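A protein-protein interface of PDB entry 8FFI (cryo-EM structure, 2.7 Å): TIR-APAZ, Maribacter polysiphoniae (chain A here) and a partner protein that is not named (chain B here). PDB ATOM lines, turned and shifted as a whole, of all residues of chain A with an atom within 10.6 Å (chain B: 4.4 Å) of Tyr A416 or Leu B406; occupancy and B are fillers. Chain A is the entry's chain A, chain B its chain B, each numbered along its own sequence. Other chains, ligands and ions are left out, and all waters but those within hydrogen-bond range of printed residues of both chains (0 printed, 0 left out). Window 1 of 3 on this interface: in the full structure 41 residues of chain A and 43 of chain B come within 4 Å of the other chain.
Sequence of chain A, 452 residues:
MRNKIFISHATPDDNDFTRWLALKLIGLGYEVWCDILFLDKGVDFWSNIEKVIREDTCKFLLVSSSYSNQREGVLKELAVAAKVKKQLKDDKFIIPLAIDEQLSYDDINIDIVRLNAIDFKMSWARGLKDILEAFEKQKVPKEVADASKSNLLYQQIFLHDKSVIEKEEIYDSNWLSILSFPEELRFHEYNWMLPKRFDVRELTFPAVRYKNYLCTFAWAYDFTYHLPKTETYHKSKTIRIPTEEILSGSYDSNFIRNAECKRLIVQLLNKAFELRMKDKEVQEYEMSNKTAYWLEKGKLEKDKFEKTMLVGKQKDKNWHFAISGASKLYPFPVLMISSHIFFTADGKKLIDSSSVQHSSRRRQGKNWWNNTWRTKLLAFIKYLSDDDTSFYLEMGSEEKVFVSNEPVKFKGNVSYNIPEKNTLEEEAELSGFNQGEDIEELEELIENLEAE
The side-chain hydroxyl (OH) of Tyr A416 sits at hydrogen-bond distance from the backbone carbonyl oxygen (O) of Thr B404. OH of Tyr A416 is in hydrogen-bond range of NZ of Lys B398, 3.1 Å away. O of Tyr B403 sits close to OH of Tyr A416 (3.3 Å). The side-chain amide oxygen (OD1) of Asn A370 is in hydrogen-bond range of the backbone NH (N) of Lys B398 (2.9 Å). The side-chain carboxylate of Glu A169 is in salt-bridge range of the side-chain amino group of Lys B398.
The side-chain amino group (NZ) of Lys A167 lies within hydrogen-bond range of the backbone carbonyl oxygen (O) of Tyr A416, at 3.4 Å. The backbone NH (N) of Arg B407 sits at hydrogen-bond distance from the backbone carbonyl oxygen (O) of Tyr B425, at 3.0 Å. The backbone carbonyl oxygen (O) of Gly A412 lies within hydrogen-bond range of the backbone NH (N) of Glu A169, 2.9 Å away. O of Ile B405 is in hydrogen-bond range of N of Tyr B425, at 3.0 Å. The side-chain carboxylate (OD1) of Asp A161 is in salt-bridge range of the side-chain amino group (NZ) of Lys A162, 3.6 Å away. O of Leu B406 lies close to OD1 of Asn B409 (3.4 Å).
Among the printed residues, merely in contact across the chains: Lys A162 with Pro B427 (3.8 Å), Ser A163 with Pro B427 (3.99 Å), Val A164 with Tyr B6 (3.5 Å), Val A164 with Leu B406 (3.7 Å), Val A164 with Pro B427 (3.7 Å), Tyr A171 with Lys B398 (3.5 Å), Tyr A171 with Ile B405 (3.9 Å), Tyr A171 with Asn B409 (3.996 Å), Asn A370 with Tyr B403 (3.6 Å), Val A414 with Tyr B6 (3.7 Å), Val A414 with Leu B406 (3.8 Å), Tyr A416 with Leu B406 (3.6 Å), Tyr A416 with Tyr B425 (3.5 Å) and Ile A418 with Tyr B403 (3.6 Å).
Of the printed residues of chain B, Val A414 touches Tyr B6 (3.7 Å) and Leu B406 (3.8 Å). Of chain B, only Lys B398 (3.1 Å), Tyr B403 (3.1 Å), Thr B404 (2.9 Å), Leu B406 (3.6 Å) and Tyr B425 (3.5 Å) come within 4 Å of Tyr A416. Of the printed residues of chain A, Tyr B6 touches Val A164 (3.5 Å) and Val A414 (3.7 Å). Of the printed residues of chain A, Ile B405 touches Tyr A171. Printed residues of chain A within 4 Å of Leu B406: Val A164 (3.7 Å), Val A414 (3.8 Å) and Tyr A416 (3.6 Å). Gly B408 touches none of the printed residues of chain A. Tyr B425 touches just one residue of chain A: Tyr A416. The nearest printed residue of chain B that does not touch Tyr A416 is Pro B427 (4.4 Å). The nearest printed residue of chain B that does not touch Glu A169 is Leu B406 (6.9 Å).
Of the 23 printed residues of chain A, 9 touch a printed residue of chain B. Printed residues of chain A that touch a printed residue of chain B: Lys A162, Ser A163, Val A164, Glu A169, Tyr A171, Asn A370, Val A414, Tyr A416 and Ile A418. Of the 11 printed residues of chain B, 9 touch a printed residue of chain A. Among the printed residues, Asp or Glu carboxylates within 4 Å of a Lys or Arg side-chain nitrogen of the other chain: Glu A169 with Lys B398 (3.96 Å).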
ATOM      1  N   ASP A 161       5.567  18.606  -3.302  1.00  0.00           N
ATOM      2  CA  ASP A 161       5.080  19.735  -4.096  1.00  0.00           C
ATOM      3  C   ASP A 161       5.603  19.688  -5.527  1.00  0.00           C
ATOM      4  O   ASP A 161       6.125  20.674  -6.046  1.00  0.00           O
ATOM      5  CB  ASP A 161       5.458  21.047  -3.419  1.00  0.00           C
ATOM      6  CG  ASP A 161       6.958  21.223  -3.282  1.00  0.00           C
ATOM      7  OD1 ASP A 161       7.664  20.204  -3.128  1.00  0.00           O
ATOM      8  OD2 ASP A 161       7.430  22.378  -3.332  1.00  0.00           O
ATOM      9  N   LYS A 162       5.452  18.549  -6.198  1.00  0.00           N
ATOM     10  CA  LYS A 162       5.929  18.388  -7.570  1.00  0.00           C
ATOM     11  C   LYS A 162       4.926  17.601  -8.397  1.00  0.00           C
ATOM     12  O   LYS A 162       5.292  16.701  -9.158  1.00  0.00           O
ATOM     13  CB  LYS A 162       7.301  17.717  -7.607  1.00  0.00           C
ATOM     14  CG  LYS A 162       8.410  18.542  -6.980  1.00  0.00           C
ATOM     15  CD  LYS A 162       9.771  17.939  -7.249  1.00  0.00           C
ATOM     16  CE  LYS A 162      10.857  18.734  -6.553  1.00  0.00           C
ATOM     17  NZ  LYS A 162      10.443  19.127  -5.180  1.00  0.00           N
ATOM     18  N   SER A 163       3.646  17.925  -8.257  1.00  0.00           N
ATOM     19  CA  SER A 163       2.576  17.240  -8.968  1.00  0.00           C
ATOM     20  C   SER A 163       1.749  18.252  -9.756  1.00  0.00           C
ATOM     21  O   SER A 163       1.987  19.460  -9.710  1.00  0.00           O
ATOM     22  CB  SER A 163       1.697  16.452  -7.993  1.00  0.00           C
ATOM     23  OG  SER A 163       2.370  15.299  -7.519  1.00  0.00           O
ATOM     24  N   VAL A 164       0.771  17.741 -10.488  1.00  0.00           N
ATOM     25  CA  VAL A 164      -0.147  18.570 -11.257  1.00  0.00           C
ATOM     26  C   VAL A 164      -1.315  18.961 -10.363  1.00  0.00           C
ATOM     27  O   VAL A 164      -1.659  18.258  -9.408  1.00  0.00           O
ATOM     28  CB  VAL A 164      -0.624  17.838 -12.527  1.00  0.00           C
ATOM     29  CG1 VAL A 164       0.516  17.712 -13.520  1.00  0.00           C
ATOM     30  CG2 VAL A 164      -1.177  16.469 -12.173  1.00  0.00           C
ATOM     31  N   ILE A 165      -1.934  20.096 -10.675  1.00  0.00           N
ATOM     32  CA  ILE A 165      -2.985  20.673  -9.848  1.00  0.00           C
ATOM     33  C   ILE A 165      -4.199  20.964 -10.717  1.00  0.00           C
ATOM     34  O   ILE A 165      -4.068  21.464 -11.838  1.00  0.00           O
ATOM     35  CB  ILE A 165      -2.502  21.956  -9.138  1.00  0.00           C
ATOM     36  CG1 ILE A 165      -1.403  21.622  -8.129  1.00  0.00           C
ATOM     37  CG2 ILE A 165      -3.654  22.666  -8.448  1.00  0.00           C
ATOM     38  CD1 ILE A 165      -0.810  22.827  -7.460  1.00  0.00           C
ATOM     39  N   GLU A 166      -5.383  20.646 -10.195  1.00  0.00           N
ATOM     40  CA  GLU A 166      -6.634  20.999 -10.855  1.00  0.00           C
ATOM     41  C   GLU A 166      -6.799  22.513 -10.827  1.00  0.00           C
ATOM     42  O   GLU A 166      -7.145  23.089  -9.790  1.00  0.00           O
ATOM     43  CB  GLU A 166      -7.806  20.309 -10.163  1.00  0.00           C
ATOM     44  CG  GLU A 166      -8.189  18.965 -10.759  1.00  0.00           C
ATOM     45  CD  GLU A 166      -9.056  19.101 -11.996  1.00  0.00           C
ATOM     46  OE1 GLU A 166     -10.245  19.454 -11.853  1.00  0.00           O
ATOM     47  OE2 GLU A 166      -8.550  18.848 -13.109  1.00  0.00           O
ATOM     48  N   LYS A 167      -6.550  23.163 -11.961  1.00  0.00           N
ATOM     49  CA  LYS A 167      -6.601  24.617 -12.041  1.00  0.00           C
ATOM     50  C   LYS A 167      -7.017  25.017 -13.446  1.00  0.00           C
ATOM     51  O   LYS A 167      -6.391  24.597 -14.424  1.00  0.00           O
ATOM     52  CB  LYS A 167      -5.247  25.237 -11.684  1.00  0.00           C
ATOM     53  CG  LYS A 167      -5.137  26.718 -12.004  1.00  0.00           C
ATOM     54  CD  LYS A 167      -4.191  27.422 -11.043  1.00  0.00           C
ATOM     55  CE  LYS A 167      -2.741  27.182 -11.421  1.00  0.00           C
ATOM     56  NZ  LYS A 167      -1.804  27.896 -10.510  1.00  0.00           N
ATOM     57  N   GLU A 168      -8.065  25.830 -13.542  1.00  0.00           N
ATOM     58  CA  GLU A 168      -8.601  26.248 -14.832  1.00  0.00           C
ATOM     59  C   GLU A 168      -7.721  27.342 -15.426  1.00  0.00           C
ATOM     60  O   GLU A 168      -7.499  28.380 -14.794  1.00  0.00           O
ATOM     61  CB  GLU A 168     -10.040  26.731 -14.667  1.00  0.00           C
ATOM     62  CG  GLU A 168     -10.791  26.934 -15.969  1.00  0.00           C
ATOM     63  CD  GLU A 168     -10.749  28.370 -16.446  1.00  0.00           C
ATOM     64  OE1 GLU A 168     -10.663  29.279 -15.594  1.00  0.00           O
ATOM     65  OE2 GLU A 168     -10.805  28.592 -17.673  1.00  0.00           O
ATOM     66  N   GLU A 169      -7.222  27.110 -16.638  1.00  0.00           N
ATOM     67  CA  GLU A 169      -6.351  28.054 -17.321  1.00  0.00           C
ATOM     68  C   GLU A 169      -6.801  28.243 -18.762  1.00  0.00           C
ATOM     69  O   GLU A 169      -7.471  27.389 -19.349  1.00  0.00           O
ATOM     70  CB  GLU A 169      -4.888  27.601 -17.295  1.00  0.00           C
ATOM     71  CG  GLU A 169      -4.247  27.674 -15.926  1.00  0.00           C
ATOM     72  CD  GLU A 169      -2.741  27.581 -15.993  1.00  0.00           C
ATOM     73  OE1 GLU A 169      -2.205  27.470 -17.114  1.00  0.00           O
ATOM     74  OE2 GLU A 169      -2.091  27.624 -14.927  1.00  0.00           O
ATOM     75  N   ILE A 170      -6.413  29.386 -19.323  1.00  0.00           N
ATOM     76  CA  ILE A 170      -6.748  29.765 -20.689  1.00  0.00           C
ATOM     77  C   ILE A 170      -5.455  30.025 -21.449  1.00  0.00           C
ATOM     78  O   ILE A 170      -4.534  30.661 -20.926  1.00  0.00           O
ATOM     79  CB  ILE A 170      -7.664  31.006 -20.725  1.00  0.00           C
ATOM     80  CG1 ILE A 170      -8.944  30.746 -19.929  1.00  0.00           C
ATOM     81  CG2 ILE A 170      -7.997  31.391 -22.157  1.00  0.00           C
ATOM     82  CD1 ILE A 170      -9.580  31.997 -19.371  1.00  0.00           C
ATOM     83  N   TYR A 171      -5.388  29.528 -22.680  1.00  0.00           N
ATOM     84  CA  TYR A 171      -4.226  29.677 -23.541  1.00  0.00           C
ATOM     85  C   TYR A 171      -4.608  30.420 -24.814  1.00  0.00           C
ATOM     86  O   TYR A 171      -5.710  30.258 -25.347  1.00  0.00           O
ATOM     87  CB  TYR A 171      -3.624  28.319 -23.927  1.00  0.00           C
ATOM     88  CG  TYR A 171      -3.332  27.385 -22.778  1.00  0.00           C
ATOM     89  CD1 TYR A 171      -4.315  26.542 -22.273  1.00  0.00           C
ATOM     90  CD2 TYR A 171      -2.068  27.328 -22.210  1.00  0.00           C
ATOM     91  CE1 TYR A 171      -4.048  25.681 -21.227  1.00  0.00           C
ATOM     92  CE2 TYR A 171      -1.793  26.472 -21.164  1.00  0.00           C
ATOM     93  CZ  TYR A 171      -2.786  25.652 -20.678  1.00  0.00           C
ATOM     94  OH  TYR A 171      -2.513  24.796 -19.637  1.00  0.00           O
ATOM     95  N   TRP A 369      11.382  33.589 -23.939  1.00  0.00           N
ATOM     96  CA  TRP A 369      10.497  32.618 -23.321  1.00  0.00           C
ATOM     97  C   TRP A 369       9.090  32.741 -23.903  1.00  0.00           C
ATOM     98  O   TRP A 369       8.861  33.426 -24.905  1.00  0.00           O
ATOM     99  CB  TRP A 369      10.504  32.794 -21.801  1.00  0.00           C
ATOM    100  CG  TRP A 369      11.878  32.834 -21.197  1.00  0.00           C
ATOM    101  CD1 TRP A 369      12.404  33.825 -20.420  1.00  0.00           C
ATOM    102  CD2 TRP A 369      12.896  31.831 -21.310  1.00  0.00           C
ATOM    103  NE1 TRP A 369      13.687  33.505 -20.048  1.00  0.00           N
ATOM    104  CE2 TRP A 369      14.014  32.286 -20.582  1.00  0.00           C
ATOM    105  CE3 TRP A 369      12.974  30.595 -21.960  1.00  0.00           C
ATOM    106  CZ2 TRP A 369      15.192  31.550 -20.486  1.00  0.00           C
ATOM    107  CZ3 TRP A 369      14.144  29.868 -21.863  1.00  0.00           C
ATOM    108  CH2 TRP A 369      15.236  30.346 -21.132  1.00  0.00           C
ATOM    109  N   ASN A 370       8.137  32.053 -23.268  1.00  0.00           N
ATOM    110  CA  ASN A 370       6.761  32.012 -23.757  1.00  0.00           C
ATOM    111  C   ASN A 370       6.166  33.413 -23.873  1.00  0.00           C
ATOM    112  O   ASN A 370       5.583  33.771 -24.907  1.00  0.00           O
ATOM    113  CB  ASN A 370       5.971  31.135 -22.782  1.00  0.00           C
ATOM    114  CG  ASN A 370       4.524  30.951 -23.186  1.00  0.00           C
ATOM    115  OD1 ASN A 370       3.728  30.345 -22.468  1.00  0.00           O
ATOM    116  ND2 ASN A 370       4.173  31.480 -24.349  1.00  0.00           N
ATOM    117  N   ASN A 371       6.299  34.216 -22.814  1.00  0.00           N
ATOM    118  CA  ASN A 371       5.647  35.521 -22.790  1.00  0.00           C
ATOM    119  C   ASN A 371       6.190  36.434 -23.880  1.00  0.00           C
ATOM    120  O   ASN A 371       5.427  37.165 -24.517  1.00  0.00           O
ATOM    121  CB  ASN A 371       5.811  36.169 -21.415  1.00  0.00           C
ATOM    122  CG  ASN A 371       4.577  36.935 -20.984  1.00  0.00           C
ATOM    123  OD1 ASN A 371       3.453  36.564 -21.322  1.00  0.00           O
ATOM    124  ND2 ASN A 371       4.779  38.011 -20.235  1.00  0.00           N
ATOM    125  N   GLY A 412      -8.301  24.726 -20.206  1.00  0.00           N
ATOM    126  CA  GLY A 412      -7.820  23.512 -19.574  1.00  0.00           C
ATOM    127  C   GLY A 412      -8.110  23.516 -18.089  1.00  0.00           C
ATOM    128  O   GLY A 412      -8.317  24.568 -17.478  1.00  0.00           O
ATOM    129  N   ASN A 413      -8.124  22.314 -17.512  1.00  0.00           N
ATOM    130  CA  ASN A 413      -8.451  22.129 -16.105  1.00  0.00           C
ATOM    131  C   ASN A 413      -7.278  21.637 -15.266  1.00  0.00           C
ATOM    132  O   ASN A 413      -7.418  21.525 -14.044  1.00  0.00           O
ATOM    133  CB  ASN A 413      -9.622  21.150 -15.962  1.00  0.00           C
ATOM    134  CG  ASN A 413     -10.908  21.688 -16.554  1.00  0.00           C
ATOM    135  OD1 ASN A 413     -11.420  21.161 -17.541  1.00  0.00           O
ATOM    136  ND2 ASN A 413     -11.443  22.741 -15.948  1.00  0.00           N
ATOM    137  N   VAL A 414      -6.135  21.340 -15.876  1.00  0.00           N
ATOM    138  CA  VAL A 414      -4.971  20.821 -15.167  1.00  0.00           C
ATOM    139  C   VAL A 414      -3.792  21.746 -15.423  1.00  0.00           C
ATOM    140  O   VAL A 414      -3.534  22.134 -16.567  1.00  0.00           O
ATOM    141  CB  VAL A 414      -4.631  19.378 -15.600  1.00  0.00           C
ATOM    142  CG1 VAL A 414      -3.475  18.837 -14.782  1.00  0.00           C
ATOM    143  CG2 VAL A 414      -5.847  18.480 -15.464  1.00  0.00           C
ATOM    144  N   SER A 415      -3.077  22.100 -14.359  1.00  0.00           N
ATOM    145  CA  SER A 415      -1.921  22.984 -14.471  1.00  0.00           C
ATOM    146  C   SER A 415      -0.968  22.695 -13.316  1.00  0.00           C
ATOM    147  O   SER A 415      -1.194  21.786 -12.511  1.00  0.00           O
ATOM    148  CB  SER A 415      -2.360  24.451 -14.494  1.00  0.00           C
ATOM    149  OG  SER A 415      -1.241  25.311 -14.611  1.00  0.00           O
ATOM    150  N   TYR A 416       0.107  23.473 -13.241  1.00  0.00           N
ATOM    151  CA  TYR A 416       1.119  23.372 -12.200  1.00  0.00           C
ATOM    152  C   TYR A 416       1.167  24.674 -11.408  1.00  0.00           C
ATOM    153  O   TYR A 416       0.507  25.659 -11.749  1.00  0.00           O
ATOM    154  CB  TYR A 416       2.495  23.031 -12.796  1.00  0.00           C
ATOM    155  CG  TYR A 416       2.939  23.932 -13.930  1.00  0.00           C
ATOM    156  CD1 TYR A 416       2.420  23.773 -15.209  1.00  0.00           C
ATOM    157  CD2 TYR A 416       3.890  24.925 -13.730  1.00  0.00           C
ATOM    158  CE1 TYR A 416       2.817  24.582 -16.247  1.00  0.00           C
ATOM    159  CE2 TYR A 416       4.296  25.742 -14.769  1.00  0.00           C
ATOM    160  CZ  TYR A 416       3.755  25.563 -16.025  1.00  0.00           C
ATOM    161  OH  TYR A 416       4.146  26.366 -17.068  1.00  0.00           O
ATOM    162  N   ASN A 417       1.966  24.676 -10.342  1.00  0.00           N
ATOM    163  CA  ASN A 417       1.907  25.732  -9.338  1.00  0.00           C
ATOM    164  C   ASN A 417       3.091  26.696  -9.457  1.00  0.00           C
ATOM    165  O   ASN A 417       3.236  27.587  -8.617  1.00  0.00           O
ATOM    166  CB  ASN A 417       1.857  25.086  -7.940  1.00  0.00           C
ATOM    167  CG  ASN A 417       1.552  26.072  -6.812  1.00  0.00           C
ATOM    168  OD1 ASN A 417       1.384  27.271  -7.023  1.00  0.00           O
ATOM    169  ND2 ASN A 417       1.473  25.548  -5.595  1.00  0.00           N
ATOM    170  N   ILE A 418       3.909  26.562 -10.500  1.00  0.00           N
ATOM    171  CA  ILE A 418       5.081  27.401 -10.784  1.00  0.00           C
ATOM    172  C   ILE A 418       5.789  27.807  -9.489  1.00  0.00           C
ATOM    173  O   ILE A 418       5.749  28.978  -9.086  1.00  0.00           O
ATOM    174  CB  ILE A 418       4.695  28.612 -11.667  1.00  0.00           C
ATOM    175  CG1 ILE A 418       5.920  29.458 -12.034  1.00  0.00           C
ATOM    176  CG2 ILE A 418       3.562  29.469 -11.073  1.00  0.00           C
ATOM    177  CD1 ILE A 418       5.640  30.501 -13.092  1.00  0.00           C
ATOM    178  N   PRO A 419       6.440  26.863  -8.786  1.00  0.00           N
ATOM    179  CA  PRO A 419       7.041  27.154  -7.478  1.00  0.00           C
ATOM    180  C   PRO A 419       8.446  27.751  -7.550  1.00  0.00           C
ATOM    181  O   PRO A 419       9.354  27.328  -6.833  1.00  0.00           O
ATOM    182  CB  PRO A 419       7.046  25.781  -6.800  1.00  0.00           C
ATOM    183  CG  PRO A 419       7.196  24.810  -7.934  1.00  0.00           C
ATOM    184  CD  PRO A 419       6.664  25.465  -9.192  1.00  0.00           C
ATOM    185  N   GLU A 420       8.614  28.754  -8.412  1.00  0.00           N
ATOM    186  CA  GLU A 420       9.873  29.484  -8.605  1.00  0.00           C
ATOM    187  C   GLU A 420      11.114  28.593  -8.574  1.00  0.00           C
ATOM    188  O   GLU A 420      11.126  27.503  -9.147  1.00  0.00           O
ATOM    189  CB  GLU A 420      10.009  30.595  -7.555  1.00  0.00           C
ATOM    190  CG  GLU A 420      10.475  30.134  -6.180  1.00  0.00           C
ATOM    191  CD  GLU A 420      10.449  31.246  -5.151  1.00  0.00           C
ATOM    192  OE1 GLU A 420       9.962  32.348  -5.477  1.00  0.00           O
ATOM    193  OE2 GLU A 420      10.913  31.016  -4.016  1.00  0.00           O
ATOM    194  N   TYR B   6      -6.582  16.159 -20.434  1.00  0.00           N
ATOM    195  CA  TYR B   6      -5.314  15.783 -19.832  1.00  0.00           C
ATOM    196  C   TYR B   6      -5.163  14.268 -19.832  1.00  0.00           C
ATOM    197  O   TYR B   6      -6.137  13.530 -19.658  1.00  0.00           O
ATOM    198  CB  TYR B   6      -5.204  16.315 -18.400  1.00  0.00           C
ATOM    199  CG  TYR B   6      -3.866  16.052 -17.751  1.00  0.00           C
ATOM    200  CD1 TYR B   6      -2.702  16.601 -18.270  1.00  0.00           C
ATOM    201  CD2 TYR B   6      -3.765  15.248 -16.626  1.00  0.00           C
ATOM    202  CE1 TYR B   6      -1.478  16.362 -17.685  1.00  0.00           C
ATOM    203  CE2 TYR B   6      -2.543  15.002 -16.034  1.00  0.00           C
ATOM    204  CZ  TYR B   6      -1.403  15.561 -16.568  1.00  0.00           C
ATOM    205  OH  TYR B   6      -0.184  15.319 -15.981  1.00  0.00           O
ATOM    206  N   LYS B 398       0.808  30.209 -22.703  1.00  0.00           N
ATOM    207  CA  LYS B 398       0.271  30.644 -21.423  1.00  0.00           C
ATOM    208  C   LYS B 398       0.293  32.165 -21.348  1.00  0.00           C
ATOM    209  O   LYS B 398       1.268  32.809 -21.741  1.00  0.00           O
ATOM    210  CB  LYS B 398       1.078  30.045 -20.272  1.00  0.00           C
ATOM    211  CG  LYS B 398       0.833  28.568 -20.040  1.00  0.00           C
ATOM    212  CD  LYS B 398       1.590  28.076 -18.819  1.00  0.00           C
ATOM    213  CE  LYS B 398       0.823  28.352 -17.540  1.00  0.00           C
ATOM    214  NZ  LYS B 398       1.632  28.054 -16.331  1.00  0.00           N
ATOM    215  N   TYR B 403       6.830  29.880 -18.650  1.00  0.00           N
ATOM    216  CA  TYR B 403       6.950  28.434 -18.750  1.00  0.00           C
ATOM    217  C   TYR B 403       5.826  27.913 -19.633  1.00  0.00           C
ATOM    218  O   TYR B 403       4.703  28.421 -19.586  1.00  0.00           O
ATOM    219  CB  TYR B 403       6.901  27.772 -17.369  1.00  0.00           C
ATOM    220  CG  TYR B 403       7.961  28.259 -16.406  1.00  0.00           C
ATOM    221  CD1 TYR B 403       9.206  28.676 -16.861  1.00  0.00           C
ATOM    222  CD2 TYR B 403       7.717  28.304 -15.040  1.00  0.00           C
ATOM    223  CE1 TYR B 403      10.176  29.123 -15.983  1.00  0.00           C
ATOM    224  CE2 TYR B 403       8.679  28.751 -14.156  1.00  0.00           C
ATOM    225  CZ  TYR B 403       9.906  29.159 -14.632  1.00  0.00           C
ATOM    226  OH  TYR B 403      10.865  29.602 -13.752  1.00  0.00           O
ATOM    227  N   THR B 404       6.133  26.900 -20.438  1.00  0.00           N
ATOM    228  CA  THR B 404       5.250  26.503 -21.522  1.00  0.00           C
ATOM    229  C   THR B 404       4.086  25.656 -21.010  1.00  0.00           C
ATOM    230  O   THR B 404       3.891  25.466 -19.807  1.00  0.00           O
ATOM    231  CB  THR B 404       6.038  25.752 -22.594  1.00  0.00           C
ATOM    232  OG1 THR B 404       6.497  24.501 -22.068  1.00  0.00           O
ATOM    233  CG2 THR B 404       7.233  26.577 -23.044  1.00  0.00           C
ATOM    234  N   ILE B 405       3.295  25.147 -21.958  1.00  0.00           N
ATOM    235  CA  ILE B 405       2.103  24.380 -21.628  1.00  0.00           C
ATOM    236  C   ILE B 405       2.491  23.063 -20.956  1.00  0.00           C
ATOM    237  O   ILE B 405       3.563  22.500 -21.207  1.00  0.00           O
ATOM    238  CB  ILE B 405       1.271  24.140 -22.900  1.00  0.00           C
ATOM    239  CG1 ILE B 405      -0.010  23.359 -22.595  1.00  0.00           C
ATOM    240  CG2 ILE B 405       2.102  23.426 -23.955  1.00  0.00           C
ATOM    241  CD1 ILE B 405      -0.859  23.081 -23.812  1.00  0.00           C
ATOM    242  N   LEU B 406       1.610  22.578 -20.082  1.00  0.00           N
ATOM    243  CA  LEU B 406       1.821  21.294 -19.429  1.00  0.00           C
ATOM    244  C   LEU B 406       1.908  20.183 -20.467  1.00  0.00           C
ATOM    245  O   LEU B 406       1.305  20.258 -21.542  1.00  0.00           O
ATOM    246  CB  LEU B 406       0.689  21.013 -18.442  1.00  0.00           C
ATOM    247  CG  LEU B 406       0.984  20.012 -17.327  1.00  0.00           C
ATOM    248  CD1 LEU B 406       2.234  20.422 -16.572  1.00  0.00           C
ATOM    249  CD2 LEU B 406      -0.200  19.904 -16.385  1.00  0.00           C
ATOM    250  N   ARG B 407       2.678  19.144 -20.141  1.00  0.00           N
ATOM    251  CA  ARG B 407       3.028  18.123 -21.121  1.00  0.00           C
ATOM    252  C   ARG B 407       1.812  17.382 -21.660  1.00  0.00           C
ATOM    253  O   ARG B 407       1.475  17.525 -22.838  1.00  0.00           O
ATOM    254  CB  ARG B 407       4.016  17.122 -20.519  1.00  0.00           C
ATOM    255  CG  ARG B 407       4.307  15.937 -21.423  1.00  0.00           C
ATOM    256  CD  ARG B 407       5.520  15.152 -20.960  1.00  0.00           C
ATOM    257  NE  ARG B 407       5.890  14.122 -21.923  1.00  0.00           N
ATOM    258  CZ  ARG B 407       5.744  12.819 -21.727  1.00  0.00           C
ATOM    259  NH1 ARG B 407       5.257  12.341 -20.593  1.00  0.00           N
ATOM    260  NH2 ARG B 407       6.098  11.973 -22.690  1.00  0.00           N
ATOM    261  N   GLY B 408       1.109  16.643 -20.810  1.00  0.00           N
ATOM    262  CA  GLY B 408       0.129  15.688 -21.297  1.00  0.00           C
ATOM    263  C   GLY B 408      -1.198  16.260 -21.757  1.00  0.00           C
ATOM    264  O   GLY B 408      -2.231  15.594 -21.644  1.00  0.00           O
ATOM    265  N   ASN B 409      -1.191  17.486 -22.269  1.00  0.00           N
ATOM    266  CA  ASN B 409      -2.410  18.103 -22.769  1.00  0.00           C
ATOM    267  C   ASN B 409      -2.709  17.637 -24.190  1.00  0.00           C
ATOM    268  O   ASN B 409      -1.806  17.289 -24.955  1.00  0.00           O
ATOM    269  CB  ASN B 409      -2.298  19.626 -22.730  1.00  0.00           C
ATOM    270  CG  ASN B 409      -2.655  20.202 -21.377  1.00  0.00           C
ATOM    271  OD1 ASN B 409      -1.928  21.027 -20.828  1.00  0.00           O
ATOM    272  ND2 ASN B 409      -3.779  19.765 -20.829  1.00  0.00           N
ATOM    273  N   TYR B 425       6.128  21.179 -20.420  1.00  0.00           N
ATOM    274  CA  TYR B 425       6.545  21.280 -19.029  1.00  0.00           C
ATOM    275  C   TYR B 425       6.214  20.003 -18.267  1.00  0.00           C
ATOM    276  O   TYR B 425       5.097  19.487 -18.347  1.00  0.00           O
ATOM    277  CB  TYR B 425       5.870  22.479 -18.365  1.00  0.00           C
ATOM    278  CG  TYR B 425       6.452  22.843 -17.021  1.00  0.00           C
ATOM    279  CD1 TYR B 425       7.546  23.692 -16.922  1.00  0.00           C
ATOM    280  CD2 TYR B 425       5.906  22.341 -15.848  1.00  0.00           C
ATOM    281  CE1 TYR B 425       8.079  24.028 -15.695  1.00  0.00           C
ATOM    282  CE2 TYR B 425       6.435  22.669 -14.619  1.00  0.00           C
ATOM    283  CZ  TYR B 425       7.521  23.511 -14.548  1.00  0.00           C
ATOM    284  OH  TYR B 425       8.046  23.843 -13.323  1.00  0.00           O
ATOM    285  N   PRO B 427       6.153  18.890 -14.385  1.00  0.00           N
ATOM    286  CA  PRO B 427       6.295  19.416 -13.016  1.00  0.00           C
ATOM    287  C   PRO B 427       7.228  18.602 -12.139  1.00  0.00           C
ATOM    288  O   PRO B 427       7.722  19.129 -11.136  1.00  0.00           O
ATOM    289  CB  PRO B 427       4.857  19.391 -12.478  1.00  0.00           C
ATOM    290  CG  PRO B 427       4.136  18.415 -13.339  1.00  0.00           C
ATOM    291  CD  PRO B 427       4.774  18.476 -14.688  1.00  0.00           C
